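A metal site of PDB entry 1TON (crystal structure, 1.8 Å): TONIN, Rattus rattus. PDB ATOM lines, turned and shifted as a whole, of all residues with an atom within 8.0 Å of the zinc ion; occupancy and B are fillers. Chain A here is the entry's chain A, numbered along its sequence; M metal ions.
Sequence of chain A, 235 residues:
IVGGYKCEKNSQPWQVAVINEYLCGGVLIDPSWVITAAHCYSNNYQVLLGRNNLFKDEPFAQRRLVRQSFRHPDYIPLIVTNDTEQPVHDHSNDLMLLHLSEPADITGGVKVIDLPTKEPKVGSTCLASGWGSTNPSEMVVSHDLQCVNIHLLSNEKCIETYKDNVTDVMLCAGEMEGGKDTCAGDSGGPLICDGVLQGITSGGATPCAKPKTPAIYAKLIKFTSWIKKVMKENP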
ATOM      1  N   HIS A  39     -20.751 -14.178  -3.650  1.00  0.00           N
ATOM      2  CA  HIS A  39     -19.964 -14.550  -4.807  1.00  0.00           C
ATOM      3  C   HIS A  39     -18.947 -13.471  -5.182  1.00  0.00           C
ATOM      4  O   HIS A  39     -18.000 -13.780  -5.901  1.00  0.00           O
ATOM      5  CB  HIS A  39     -20.830 -14.712  -6.116  1.00  0.00           C
ATOM      6  CG  HIS A  39     -21.388 -16.071  -6.363  1.00  0.00           C
ATOM      7  ND1 HIS A  39     -22.695 -16.413  -6.038  1.00  0.00           N
ATOM      8  CD2 HIS A  39     -20.863 -17.180  -6.959  1.00  0.00           C
ATOM      9  CE1 HIS A  39     -22.915 -17.688  -6.341  1.00  0.00           C
ATOM     10  NE2 HIS A  39     -21.813 -18.163  -6.927  1.00  0.00           N
ATOM     11  N   TYR A  75     -23.085 -19.429   3.664  1.00  0.00           N
ATOM     12  CA  TYR A  75     -22.673 -19.484   2.237  1.00  0.00           C
ATOM     13  C   TYR A  75     -21.471 -20.432   2.117  1.00  0.00           C
ATOM     14  O   TYR A  75     -20.466 -20.243   2.820  1.00  0.00           O
ATOM     15  CB  TYR A  75     -22.322 -18.102   1.711  1.00  0.00           C
ATOM     16  CG  TYR A  75     -21.905 -18.120   0.249  1.00  0.00           C
ATOM     17  CD1 TYR A  75     -20.556 -17.886  -0.080  1.00  0.00           C
ATOM     18  CD2 TYR A  75     -22.807 -18.349  -0.769  1.00  0.00           C
ATOM     19  CE1 TYR A  75     -20.130 -17.890  -1.393  1.00  0.00           C
ATOM     20  CE2 TYR A  75     -22.394 -18.336  -2.103  1.00  0.00           C
ATOM     21  CZ  TYR A  75     -21.073 -18.021  -2.406  1.00  0.00           C
ATOM     22  OH  TYR A  75     -20.754 -18.088  -3.762  1.00  0.00           O
ATOM     23  N   ILE A  76     -21.534 -21.341   1.161  1.00  0.00           N
ATOM     24  CA  ILE A  76     -20.456 -22.268   0.839  1.00  0.00           C
ATOM     25  C   ILE A  76     -19.820 -21.782  -0.497  1.00  0.00           C
ATOM     26  O   ILE A  76     -20.493 -21.982  -1.521  1.00  0.00           O
ATOM     27  CB  ILE A  76     -20.899 -23.742   0.552  1.00  0.00           C
ATOM     28  CG1 ILE A  76     -21.305 -24.441   1.879  1.00  0.00           C
ATOM     29  CG2 ILE A  76     -19.810 -24.517  -0.224  1.00  0.00           C
ATOM     30  CD1 ILE A  76     -22.711 -25.105   1.635  1.00  0.00           C
ATOM     31  N   PRO A  77     -18.624 -21.288  -0.373  1.00  0.00           N
ATOM     32  CA  PRO A  77     -17.896 -20.779  -1.542  1.00  0.00           C
ATOM     33  C   PRO A  77     -17.604 -21.819  -2.606  1.00  0.00           C
ATOM     34  O   PRO A  77     -17.485 -23.059  -2.387  1.00  0.00           O
ATOM     35  CB  PRO A  77     -16.620 -20.156  -0.962  1.00  0.00           C
ATOM     36  CG  PRO A  77     -16.901 -19.964   0.511  1.00  0.00           C
ATOM     37  CD  PRO A  77     -17.915 -21.041   0.900  1.00  0.00           C
ATOM     38  N   LEU A  78     -17.563 -21.262  -3.821  1.00  0.00           N
ATOM     39  CA  LEU A  78     -17.104 -22.047  -5.012  1.00  0.00           C
ATOM     40  C   LEU A  78     -15.564 -22.163  -4.711  1.00  0.00           C
ATOM     41  O   LEU A  78     -14.960 -21.050  -4.665  1.00  0.00           O
ATOM     42  CB  LEU A  78     -17.392 -21.322  -6.295  1.00  0.00           C
ATOM     43  CG  LEU A  78     -17.324 -21.925  -7.666  1.00  0.00           C
ATOM     44  CD1 LEU A  78     -18.660 -22.601  -7.995  1.00  0.00           C
ATOM     45  CD2 LEU A  78     -17.094 -20.864  -8.727  1.00  0.00           C
ATOM     46  N   HIS A  89     -20.791 -26.232  -3.206  1.00  0.00           N
ATOM     47  CA  HIS A  89     -21.195 -24.877  -3.437  1.00  0.00           C
ATOM     48  C   HIS A  89     -22.610 -24.837  -4.024  1.00  0.00           C
ATOM     49  O   HIS A  89     -22.848 -25.582  -5.005  1.00  0.00           O
ATOM     50  CB  HIS A  89     -20.268 -24.246  -4.551  1.00  0.00           C
ATOM     51  CG  HIS A  89     -20.715 -22.902  -4.990  1.00  0.00           C
ATOM     52  ND1 HIS A  89     -20.601 -21.763  -4.201  1.00  0.00           N
ATOM     53  CD2 HIS A  89     -21.265 -22.502  -6.170  1.00  0.00           C
ATOM     54  CE1 HIS A  89     -21.071 -20.746  -4.883  1.00  0.00           C
ATOM     55  NE2 HIS A  89     -21.474 -21.139  -6.057  1.00  0.00           N
ATOM     56  N   ASP A  90     -23.446 -23.952  -3.493  1.00  0.00           N
ATOM     57  CA  ASP A  90     -24.785 -23.787  -4.095  1.00  0.00           C
ATOM     58  C   ASP A  90     -25.008 -22.265  -3.996  1.00  0.00           C
ATOM     59  O   ASP A  90     -24.117 -21.561  -3.507  1.00  0.00           O
ATOM     60  CB  ASP A  90     -25.869 -24.673  -3.531  1.00  0.00           C
ATOM     61  CG  ASP A  90     -26.163 -24.492  -2.054  1.00  0.00           C
ATOM     62  OD1 ASP A  90     -26.276 -23.340  -1.583  1.00  0.00           O
ATOM     63  OD2 ASP A  90     -26.280 -25.501  -1.304  1.00  0.00           O
ATOM     64  N   HIS A  91     -26.143 -21.888  -4.459  1.00  0.00           N
ATOM     65  CA  HIS A  91     -26.460 -20.412  -4.446  1.00  0.00           C
ATOM     66  C   HIS A  91     -27.372 -20.045  -3.335  1.00  0.00           C
ATOM     67  O   HIS A  91     -27.789 -18.840  -3.330  1.00  0.00           O
ATOM     68  CB  HIS A  91     -26.908 -20.022  -5.834  1.00  0.00           C
ATOM     69  CG  HIS A  91     -25.769 -20.118  -6.817  1.00  0.00           C
ATOM     70  ND1 HIS A  91     -25.982 -19.844  -8.153  1.00  0.00           N
ATOM     71  CD2 HIS A  91     -24.460 -20.377  -6.664  1.00  0.00           C
ATOM     72  CE1 HIS A  91     -24.826 -19.998  -8.800  1.00  0.00           C
ATOM     73  NE2 HIS A  91     -23.878 -20.282  -7.925  1.00  0.00           N
ATOM     74  N   SER A  92     -27.601 -20.880  -2.341  1.00  0.00           N
ATOM     75  CA  SER A  92     -28.397 -20.537  -1.164  1.00  0.00           C
ATOM     76  C   SER A  92     -27.474 -19.703  -0.274  1.00  0.00           C
ATOM     77  O   SER A  92     -26.227 -19.903  -0.296  1.00  0.00           O
ATOM     78  CB  SER A  92     -28.910 -21.801  -0.415  1.00  0.00           C
ATOM     79  OG  SER A  92     -27.886 -22.368   0.389  1.00  0.00           O
ATOM     80  N   ASP A  94     -26.526 -16.669  -0.586  1.00  0.00           N
ATOM     81  CA  ASP A  94     -25.579 -15.845  -1.369  1.00  0.00           C
ATOM     82  C   ASP A  94     -25.782 -14.359  -1.017  1.00  0.00           C
ATOM     83  O   ASP A  94     -26.339 -13.581  -1.808  1.00  0.00           O
ATOM     84  CB  ASP A  94     -25.725 -16.154  -2.844  1.00  0.00           C
ATOM     85  CG  ASP A  94     -24.628 -15.453  -3.680  1.00  0.00           C
ATOM     86  OD1 ASP A  94     -23.602 -15.133  -3.111  1.00  0.00           O
ATOM     87  OD2 ASP A  94     -24.907 -15.336  -4.899  1.00  0.00           O
ATOM     88  N   SER A 187     -24.978 -10.114 -10.443  1.00  0.00           N
ATOM     89  CA  SER A 187     -25.009 -10.681  -9.113  1.00  0.00           C
ATOM     90  C   SER A 187     -24.958  -9.610  -8.027  1.00  0.00           C
ATOM     91  O   SER A 187     -24.107  -8.716  -8.181  1.00  0.00           O
ATOM     92  CB  SER A 187     -23.776 -11.599  -8.938  1.00  0.00           C
ATOM     93  OG  SER A 187     -24.007 -12.777  -9.706  1.00  0.00           O
ATOM     94  N   SER A 202     -28.399 -13.727  -7.475  1.00  0.00           N
ATOM     95  CA  SER A 202     -27.319 -14.667  -7.172  1.00  0.00           C
ATOM     96  C   SER A 202     -26.403 -14.793  -8.398  1.00  0.00           C
ATOM     97  O   SER A 202     -26.408 -13.910  -9.319  1.00  0.00           O
ATOM     98  CB  SER A 202     -27.806 -16.012  -6.666  1.00  0.00           C
ATOM     99  OG  SER A 202     -26.653 -16.801  -6.213  1.00  0.00           O
ATOM    100  N   GLY A 203     -25.590 -15.833  -8.399  1.00  0.00           N
ATOM    101  CA  GLY A 203     -24.639 -16.096  -9.501  1.00  0.00           C
ATOM    102  C   GLY A 203     -25.406 -16.250 -10.815  1.00  0.00           C
ATOM    103  O   GLY A 203     -26.363 -17.057 -10.831  1.00  0.00           O
ATOM    104  N   GLY A 204     -25.021 -15.527 -11.858  1.00  0.00           N
ATOM    105  CA  GLY A 204     -25.691 -15.603 -13.172  1.00  0.00           C
ATOM    106  C   GLY A 204     -24.761 -15.922 -14.321  1.00  0.00           C
ATOM    107  O   GLY A 204     -24.588 -15.139 -15.290  1.00  0.00           O
ATOM    108  N   ALA A 205     -24.204 -17.131 -14.281  1.00  0.00           N
ATOM    109  CA  ALA A 205     -23.273 -17.641 -15.315  1.00  0.00           C
ATOM    110  C   ALA A 205     -23.987 -17.762 -16.644  1.00  0.00           C
ATOM    111  O   ALA A 205     -25.221 -18.019 -16.670  1.00  0.00           O
ATOM    112  CB  ALA A 205     -22.789 -19.016 -14.815  1.00  0.00           C
HETATM  113 ZN    ZN M   1     -21.842 -20.034  -7.742  1.00  0.00          ZN
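A ring nitrogen (ND1) of His 89 is in hydrogen-bond range of the backbone carbonyl oxygen (O) of Ile 76 (2.7 Å).
A ring nitrogen (ND1) of His 89 sits at hydrogen-bond distance from the backbone NH of Leu 78 (3.1 Å).
A ring nitrogen (ND1) of His 39 sits at hydrogen-bond distance from the side-chain carboxylate of Asp 94 (2.7 Å).
A ring nitrogen (ND1) of His 39 sits close to the side-chain hydroxyl (OH) of Tyr 75 (3.4 Å).
Three residues have an atom within 4 Å of the zinc ion: His 39, His 89 and His 91.
The nearest printed residue that does not touch the zinc ion is Leu 78 (4.1 Å).
The zinc ion is bound by a ring nitrogen (NE2) of His 39, a ring nitrogen (NE2) of His 89 and a ring nitrogen (NE2) of His 91.
The zinc ion has three donor atoms within binding distance.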
